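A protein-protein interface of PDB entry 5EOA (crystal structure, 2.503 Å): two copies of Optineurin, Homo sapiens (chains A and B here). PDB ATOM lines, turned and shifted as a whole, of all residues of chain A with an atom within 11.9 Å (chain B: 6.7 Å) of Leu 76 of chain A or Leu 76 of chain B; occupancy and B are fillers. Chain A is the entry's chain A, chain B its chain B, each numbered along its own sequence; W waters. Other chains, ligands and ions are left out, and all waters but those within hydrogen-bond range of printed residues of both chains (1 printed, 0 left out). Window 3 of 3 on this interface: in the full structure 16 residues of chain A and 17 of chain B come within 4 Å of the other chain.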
ATOM      1  N   ILE A  67      19.969  13.549  13.391  1.00  0.00           N
ATOM      2  CA  ILE A  67      20.889  12.566  12.826  1.00  0.00           C
ATOM      3  C   ILE A  67      20.861  12.607  11.303  1.00  0.00           C
ATOM      4  O   ILE A  67      21.915  12.589  10.660  1.00  0.00           O
ATOM      5  CB  ILE A  67      20.571  11.140  13.321  1.00  0.00           C
ATOM      6  CG1 ILE A  67      21.242  10.896  14.667  1.00  0.00           C
ATOM      7  CG2 ILE A  67      21.032  10.085  12.324  1.00  0.00           C
ATOM      8  CD1 ILE A  67      20.892   9.562  15.280  1.00  0.00           C
ATOM      9  N   GLN A  68      19.662  12.666  10.727  1.00  0.00           N
ATOM     10  CA  GLN A  68      19.533  12.700   9.272  1.00  0.00           C
ATOM     11  C   GLN A  68      20.186  13.945   8.683  1.00  0.00           C
ATOM     12  O   GLN A  68      20.749  13.905   7.584  1.00  0.00           O
ATOM     13  CB  GLN A  68      18.071  12.601   8.841  1.00  0.00           C
ATOM     14  CG  GLN A  68      17.539  11.185   8.810  1.00  0.00           C
ATOM     15  CD  GLN A  68      16.891  10.843   7.481  1.00  0.00           C
ATOM     16  OE1 GLN A  68      16.252  11.694   6.859  1.00  0.00           O
ATOM     17  NE2 GLN A  68      17.058   9.594   7.034  1.00  0.00           N
ATOM     18  N   SER A  69      20.135  15.038   9.433  1.00  0.00           N
ATOM     19  CA  SER A  69      20.672  16.309   8.971  1.00  0.00           C
ATOM     20  C   SER A  69      22.190  16.263   8.928  1.00  0.00           C
ATOM     21  O   SER A  69      22.802  16.693   7.958  1.00  0.00           O
ATOM     22  CB  SER A  69      20.220  17.441   9.892  1.00  0.00           C
ATOM     23  OG  SER A  69      20.236  18.681   9.211  1.00  0.00           O
ATOM     24  N   LYS A  70      22.790  15.730   9.984  1.00  0.00           N
ATOM     25  CA  LYS A  70      24.232  15.662  10.067  1.00  0.00           C
ATOM     26  C   LYS A  70      24.775  14.689   9.035  1.00  0.00           C
ATOM     27  O   LYS A  70      25.841  14.913   8.458  1.00  0.00           O
ATOM     28  CB  LYS A  70      24.681  15.268  11.470  1.00  0.00           C
ATOM     29  CG  LYS A  70      24.932  16.463  12.375  1.00  0.00           C
ATOM     30  CD  LYS A  70      25.977  16.137  13.433  1.00  0.00           C
ATOM     31  CE  LYS A  70      25.395  15.309  14.558  1.00  0.00           C
ATOM     32  NZ  LYS A  70      24.410  16.096  15.340  1.00  0.00           N
ATOM     33  N   GLU A  71      24.035  13.616   8.793  1.00  0.00           N
ATOM     34  CA  GLU A  71      24.475  12.628   7.831  1.00  0.00           C
ATOM     35  C   GLU A  71      24.346  13.157   6.412  1.00  0.00           C
ATOM     36  O   GLU A  71      25.097  12.772   5.528  1.00  0.00           O
ATOM     37  CB  GLU A  71      23.719  11.319   8.016  1.00  0.00           C
ATOM     38  CG  GLU A  71      24.152  10.574   9.277  1.00  0.00           C
ATOM     39  CD  GLU A  71      23.542   9.191   9.384  1.00  0.00           C
ATOM     40  OE1 GLU A  71      22.617   8.886   8.603  1.00  0.00           O
ATOM     41  OE2 GLU A  71      23.989   8.407  10.247  1.00  0.00           O
ATOM     42  N   ALA A  72      23.408  14.061   6.185  1.00  0.00           N
ATOM     43  CA  ALA A  72      23.293  14.657   4.865  1.00  0.00           C
ATOM     44  C   ALA A  72      24.416  15.666   4.668  1.00  0.00           C
ATOM     45  O   ALA A  72      24.852  15.910   3.549  1.00  0.00           O
ATOM     46  CB  ALA A  72      21.955  15.329   4.706  1.00  0.00           C
ATOM     47  N   LYS A  73      24.867  16.257   5.771  1.00  0.00           N
ATOM     48  CA  LYS A  73      25.853  17.327   5.730  1.00  0.00           C
ATOM     49  C   LYS A  73      27.258  16.782   5.521  1.00  0.00           C
ATOM     50  O   LYS A  73      27.978  17.261   4.652  1.00  0.00           O
ATOM     51  CB  LYS A  73      25.781  18.194   7.001  1.00  0.00           C
ATOM     52  CG  LYS A  73      24.710  19.283   6.961  1.00  0.00           C
ATOM     53  CD  LYS A  73      24.615  20.043   8.295  1.00  0.00           C
ATOM     54  CE  LYS A  73      23.267  20.791   8.438  1.00  0.00           C
ATOM     55  NZ  LYS A  73      23.236  21.681   9.636  1.00  0.00           N
ATOM     56  N   GLU A  74      27.646  15.784   6.307  1.00  0.00           N
ATOM     57  CA  GLU A  74      28.977  15.193   6.162  1.00  0.00           C
ATOM     58  C   GLU A  74      29.112  14.448   4.838  1.00  0.00           C
ATOM     59  O   GLU A  74      30.187  14.430   4.235  1.00  0.00           O
ATOM     60  CB  GLU A  74      29.319  14.273   7.341  1.00  0.00           C
ATOM     61  CG  GLU A  74      28.546  12.956   7.383  1.00  0.00           C
ATOM     62  CD  GLU A  74      28.689  12.236   8.720  1.00  0.00           C
ATOM     63  OE1 GLU A  74      29.492  12.697   9.566  1.00  0.00           O
ATOM     64  OE2 GLU A  74      27.993  11.213   8.926  1.00  0.00           O
ATOM     65  N   ARG A  75      28.017  13.849   4.383  1.00  0.00           N
ATOM     66  CA  ARG A  75      28.021  13.066   3.154  1.00  0.00           C
ATOM     67  C   ARG A  75      28.122  13.986   1.950  1.00  0.00           C
ATOM     68  O   ARG A  75      28.707  13.627   0.922  1.00  0.00           O
ATOM     69  CB  ARG A  75      26.763  12.206   3.097  1.00  0.00           C
ATOM     70  CG  ARG A  75      26.330  11.709   1.738  1.00  0.00           C
ATOM     71  CD  ARG A  75      25.045  10.911   1.915  1.00  0.00           C
ATOM     72  NE  ARG A  75      24.356  10.609   0.663  1.00  0.00           N
ATOM     73  CZ  ARG A  75      23.134  10.086   0.598  1.00  0.00           C
ATOM     74  NH1 ARG A  75      22.576   9.842  -0.582  1.00  0.00           N
ATOM     75  NH2 ARG A  75      22.466   9.809   1.716  1.00  0.00           N
ATOM     76  N   LEU A  76      27.565  15.184   2.090  1.00  0.00           N
ATOM     77  CA  LEU A  76      27.714  16.217   1.071  1.00  0.00           C
ATOM     78  C   LEU A  76      29.176  16.627   0.972  1.00  0.00           C
ATOM     79  O   LEU A  76      29.778  16.585  -0.103  1.00  0.00           O
ATOM     80  CB  LEU A  76      26.859  17.430   1.424  1.00  0.00           C
ATOM     81  CG  LEU A  76      27.087  18.714   0.631  1.00  0.00           C
ATOM     82  CD1 LEU A  76      26.883  18.465  -0.851  1.00  0.00           C
ATOM     83  CD2 LEU A  76      26.155  19.814   1.126  1.00  0.00           C
ATOM     84  N   MET A  77      29.740  17.009   2.113  1.00  0.00           N
ATOM     85  CA  MET A  77      31.127  17.441   2.139  1.00  0.00           C
ATOM     86  C   MET A  77      32.093  16.279   1.868  1.00  0.00           C
ATOM     87  O   MET A  77      33.258  16.502   1.535  1.00  0.00           O
ATOM     88  CB  MET A  77      31.440  18.178   3.442  1.00  0.00           C
ATOM     89  CG  MET A  77      30.378  19.221   3.789  1.00  0.00           C
ATOM     90  SD  MET A  77      30.975  20.734   4.573  1.00  0.00           S
ATOM     91  CE  MET A  77      31.789  20.091   6.038  1.00  0.00           C
ATOM     92  N   ALA A  78      31.596  15.047   1.939  1.00  0.00           N
ATOM     93  CA  ALA A  78      32.419  13.883   1.610  1.00  0.00           C
ATOM     94  C   ALA A  78      32.846  13.852   0.142  1.00  0.00           C
ATOM     95  O   ALA A  78      33.740  13.086  -0.230  1.00  0.00           O
ATOM     96  CB  ALA A  78      31.702  12.596   1.976  1.00  0.00           C
ATOM     97  N   LEU A  79      32.219  14.679  -0.693  1.00  0.00           N
ATOM     98  CA  LEU A  79      32.620  14.779  -2.101  1.00  0.00           C
ATOM     99  C   LEU A  79      32.652  16.230  -2.602  1.00  0.00           C
ATOM    100  O   LEU A  79      31.611  16.893  -2.656  1.00  0.00           O
ATOM    101  CB  LEU A  79      31.719  13.898  -2.986  1.00  0.00           C
ATOM    102  CG  LEU A  79      30.395  13.401  -2.372  1.00  0.00           C
ATOM    103  CD1 LEU A  79      29.316  14.466  -2.468  1.00  0.00           C
ATOM    104  CD2 LEU A  79      29.911  12.092  -3.002  1.00  0.00           C
ATOM    105  N   SER A  80      33.841  16.732  -2.944  1.00  0.00           N
ATOM    106  CA  SER A  80      35.091  15.994  -2.797  1.00  0.00           C
ATOM    107  C   SER A  80      35.934  16.606  -1.684  1.00  0.00           C
ATOM    108  O   SER A  80      35.513  16.671  -0.529  1.00  0.00           O
ATOM    109  CB  SER A  80      35.886  15.989  -4.112  1.00  0.00           C
ATOM    110  OG  SER A  80      36.680  17.159  -4.270  1.00  0.00           O
ATOM    111  N   GLU B  71      16.204  20.621   4.062  1.00  0.00           N
ATOM    112  CA  GLU B  71      17.112  21.459   3.310  1.00  0.00           C
ATOM    113  C   GLU B  71      18.459  20.768   3.041  1.00  0.00           C
ATOM    114  O   GLU B  71      18.995  20.863   1.936  1.00  0.00           O
ATOM    115  CB  GLU B  71      17.275  22.812   4.000  1.00  0.00           C
ATOM    116  CG  GLU B  71      16.055  23.702   3.806  1.00  0.00           C
ATOM    117  CD  GLU B  71      16.137  25.025   4.546  1.00  0.00           C
ATOM    118  OE1 GLU B  71      17.201  25.334   5.119  1.00  0.00           O
ATOM    119  OE2 GLU B  71      15.131  25.765   4.561  1.00  0.00           O
ATOM    120  N   ALA B  72      18.995  20.068   4.038  1.00  0.00           N
ATOM    121  CA  ALA B  72      20.251  19.351   3.857  1.00  0.00           C
ATOM    122  C   ALA B  72      20.125  18.304   2.740  1.00  0.00           C
ATOM    123  O   ALA B  72      21.066  18.088   1.952  1.00  0.00           O
ATOM    124  CB  ALA B  72      20.697  18.707   5.150  1.00  0.00           C
ATOM    125  N   LYS B  73      18.955  17.675   2.666  1.00  0.00           N
ATOM    126  CA  LYS B  73      18.713  16.638   1.679  1.00  0.00           C
ATOM    127  C   LYS B  73      18.512  17.267   0.300  1.00  0.00           C
ATOM    128  O   LYS B  73      19.022  16.756  -0.697  1.00  0.00           O
ATOM    129  CB  LYS B  73      17.510  15.770   2.077  1.00  0.00           C
ATOM    130  CG  LYS B  73      17.746  14.872   3.300  1.00  0.00           C
ATOM    131  CD  LYS B  73      16.438  14.292   3.855  1.00  0.00           C
ATOM    132  CE  LYS B  73      16.193  12.852   3.397  1.00  0.00           C
ATOM    133  NZ  LYS B  73      17.104  11.846   4.034  1.00  0.00           N
ATOM    134  N   GLU B  74      17.776  18.375   0.248  1.00  0.00           N
ATOM    135  CA  GLU B  74      17.572  19.091  -1.001  1.00  0.00           C
ATOM    136  C   GLU B  74      18.927  19.472  -1.570  1.00  0.00           C
ATOM    137  O   GLU B  74      19.198  19.264  -2.754  1.00  0.00           O
ATOM    138  CB  GLU B  74      16.724  20.347  -0.786  1.00  0.00           C
ATOM    139  CG  GLU B  74      15.223  20.125  -0.703  1.00  0.00           C
ATOM    140  CD  GLU B  74      14.511  21.288  -0.016  1.00  0.00           C
ATOM    141  OE1 GLU B  74      15.160  22.335   0.204  1.00  0.00           O
ATOM    142  OE2 GLU B  74      13.310  21.155   0.318  1.00  0.00           O
ATOM    143  N   ARG B  75      19.781  20.015  -0.710  1.00  0.00           N
ATOM    144  CA  ARG B  75      21.120  20.442  -1.103  1.00  0.00           C
ATOM    145  C   ARG B  75      21.950  19.254  -1.589  1.00  0.00           C
ATOM    146  O   ARG B  75      22.677  19.353  -2.575  1.00  0.00           O
ATOM    147  CB  ARG B  75      21.807  21.165   0.061  1.00  0.00           C
ATOM    148  CG  ARG B  75      23.249  21.575  -0.184  1.00  0.00           C
ATOM    149  CD  ARG B  75      23.749  22.496   0.924  1.00  0.00           C
ATOM    150  NE  ARG B  75      22.902  23.677   1.060  1.00  0.00           N
ATOM    151  CZ  ARG B  75      23.066  24.801   0.365  1.00  0.00           C
ATOM    152  NH1 ARG B  75      22.243  25.822   0.559  1.00  0.00           N
ATOM    153  NH2 ARG B  75      24.053  24.911  -0.521  1.00  0.00           N
ATOM    154  N   LEU B  76      21.809  18.128  -0.905  1.00  0.00           N
ATOM    155  CA  LEU B  76      22.518  16.918  -1.282  1.00  0.00           C
ATOM    156  C   LEU B  76      22.117  16.484  -2.685  1.00  0.00           C
ATOM    157  O   LEU B  76      22.973  16.154  -3.502  1.00  0.00           O
ATOM    158  CB  LEU B  76      22.203  15.802  -0.289  1.00  0.00           C
ATOM    159  CG  LEU B  76      23.384  15.018   0.278  1.00  0.00           C
ATOM    160  CD1 LEU B  76      22.981  13.574   0.490  1.00  0.00           C
ATOM    161  CD2 LEU B  76      24.589  15.112  -0.632  1.00  0.00           C
ATOM    162  N   MET B  77      20.816  16.499  -2.960  1.00  0.00           N
ATOM    163  CA  MET B  77      20.309  16.148  -4.279  1.00  0.00           C
ATOM    164  C   MET B  77      20.790  17.117  -5.354  1.00  0.00           C
ATOM    165  O   MET B  77      21.343  16.694  -6.362  1.00  0.00           O
ATOM    166  CB  MET B  77      18.780  16.085  -4.281  1.00  0.00           C
ATOM    167  CG  MET B  77      18.191  14.823  -3.658  1.00  0.00           C
ATOM    168  SD  MET B  77      18.023  13.435  -4.808  1.00  0.00           S
ATOM    169  CE  MET B  77      19.692  12.784  -4.884  1.00  0.00           C
ATOM    170  N   ALA B  78      20.591  18.413  -5.133  1.00  0.00           N
ATOM    171  CA  ALA B  78      20.919  19.430  -6.134  1.00  0.00           C
ATOM    172  C   ALA B  78      22.397  19.505  -6.491  1.00  0.00           C
ATOM    173  O   ALA B  78      22.750  19.900  -7.608  1.00  0.00           O
ATOM    174  CB  ALA B  78      20.438  20.794  -5.678  1.00  0.00           C
ATOM    175  N   LEU B  79      23.254  19.141  -5.542  1.00  0.00           N
ATOM    176  CA  LEU B  79      24.687  19.370  -5.687  1.00  0.00           C
ATOM    177  C   LEU B  79      25.440  18.097  -6.061  1.00  0.00           C
ATOM    178  O   LEU B  79      26.643  18.131  -6.296  1.00  0.00           O
ATOM    179  CB  LEU B  79      25.264  20.006  -4.411  1.00  0.00           C
ATOM    180  CG  LEU B  79      25.476  21.531  -4.411  1.00  0.00           C
ATOM    181  CD1 LEU B  79      24.365  22.271  -5.131  1.00  0.00           C
ATOM    182  CD2 LEU B  79      25.633  22.070  -3.002  1.00  0.00           C
ATOM    183  N   SER B  80      24.716  16.980  -6.111  1.00  0.00           N
ATOM    184  CA  SER B  80      25.256  15.709  -6.592  1.00  0.00           C
ATOM    185  C   SER B  80      24.932  15.504  -8.076  1.00  0.00           C
ATOM    186  O   SER B  80      25.775  15.038  -8.842  1.00  0.00           O
ATOM    187  CB  SER B  80      24.708  14.543  -5.762  1.00  0.00           C
ATOM    188  OG  SER B  80      23.302  14.405  -5.906  1.00  0.00           O
ATOM    189  N   HIS B  81      23.711  15.865  -8.476  1.00  0.00           N
ATOM    190  CA  HIS B  81      23.291  15.804  -9.879  1.00  0.00           C
ATOM    191  C   HIS B  81      23.968  16.893 -10.702  1.00  0.00           C
ATOM    192  O   HIS B  81      24.905  17.546 -10.244  1.00  0.00           O
ATOM    193  CB  HIS B  81      21.768  15.948 -10.011  1.00  0.00           C
ATOM    194  CG  HIS B  81      21.002  14.693  -9.710  1.00  0.00           C
ATOM    195  ND1 HIS B  81      21.259  13.903  -8.609  1.00  0.00           N
ATOM    196  CD2 HIS B  81      19.970  14.105 -10.362  1.00  0.00           C
ATOM    197  CE1 HIS B  81      20.424  12.878  -8.600  1.00  0.00           C
ATOM    198  NE2 HIS B  81      19.631  12.978  -9.652  1.00  0.00           N
HETATM  199  O   HOH W   1      23.958  18.465   2.804  1.00  0.00           O
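The side-chain amide oxygen (OE1) of Gln 68 of chain A is in hydrogen-bond range of the side-chain amino group (NZ) of Lys 73 of chain B (3.0 Å).
The backbone carbonyl oxygen of Leu 76 of chain B sits at hydrogen-bond distance from the side-chain hydroxyl of Ser 80 of chain B.
Among the printed residues, merely in contact across the chains: Arg 75 of chain A with Leu 76 of chain B (3.3 Å), Leu 76 of chain A with Arg 75 of chain B (3.6 Å), Ala 72 of chain A with Ala 72 of chain B (3.6 Å), Ala 72 of chain A with Leu 76 of chain B (3.7 Å) and Leu 76 of chain A with Leu 76 of chain B (3.7 Å).
Of the printed residues of chain B, Ala 72 of chain A touches Ala 72 (3.6 Å) and Leu 76 (3.7 Å). Of the printed residues of chain B, Arg 75 of chain A touches Leu 76 (3.3 Å). Of chain B, only Arg 75 and Leu 76 come within 4 Å of Leu 76 of chain A. Leu 79 of chain A touches none of the printed residues of chain B. Ser 80 of chain A touches none of the printed residues of chain B. Of the printed residues of chain A, Lys 73 of chain B touches Gln 68. Of chain A, only Leu 76 (3.6 Å) comes within 4 Å of Arg 75 of chain B. Of chain A, only Ala 72, Arg 75 and Leu 76 come within 4 Å of Leu 76 of chain B. Met 77 of chain B touches none of the printed residues of chain A. No residue of chain A comes within 4 Å of Leu 79 of chain B. No residue of chain A comes within 4 Å of Ser 80 of chain B. No residue of chain A comes within 4 Å of His 81 of chain B. The nearest residue of chain B that does not touch Leu 76 of chain A is Leu 79 of chain B (4.2 Å).
Hydrophobic or aromatic side chains of chain A within 4 Å of the printed part of chain B: Ala 72 and Leu 76. Among the printed residues, 6 pairs touch across the chains. Among the printed residues, no Asp or Glu carboxylate lies within 4 Å of a Lys or Arg side-chain nitrogen of the other chain.
Ala 72 of chain A touches its own counterpart, Ala 72 of chain B. Ala 72 of chain A touches Leu 76 of chain B, but with the chains exchanged Leu 76 of chain A does not touch Ala 72 of chain B (5.4 Å). Arg 75 of chain A touches Leu 76 of chain B, and with the chains exchanged Leu 76 of chain A touches Arg 75 of chain B. Leu 76 of chain A touches its own counterpart, Leu 76 of chain B. Positions printed for both chains: 71, 72, 73, 74, 75, 76, 77, 78, 79 and 80. Of the 6 pairs that touch across the chains among the printed residues, 4 have their exchanged pair printed and touching as well.
Water W1 bridges O of Ala 72 of chain A (2.8 Å) and O of Ala 72 of chain B (3.0 Å).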
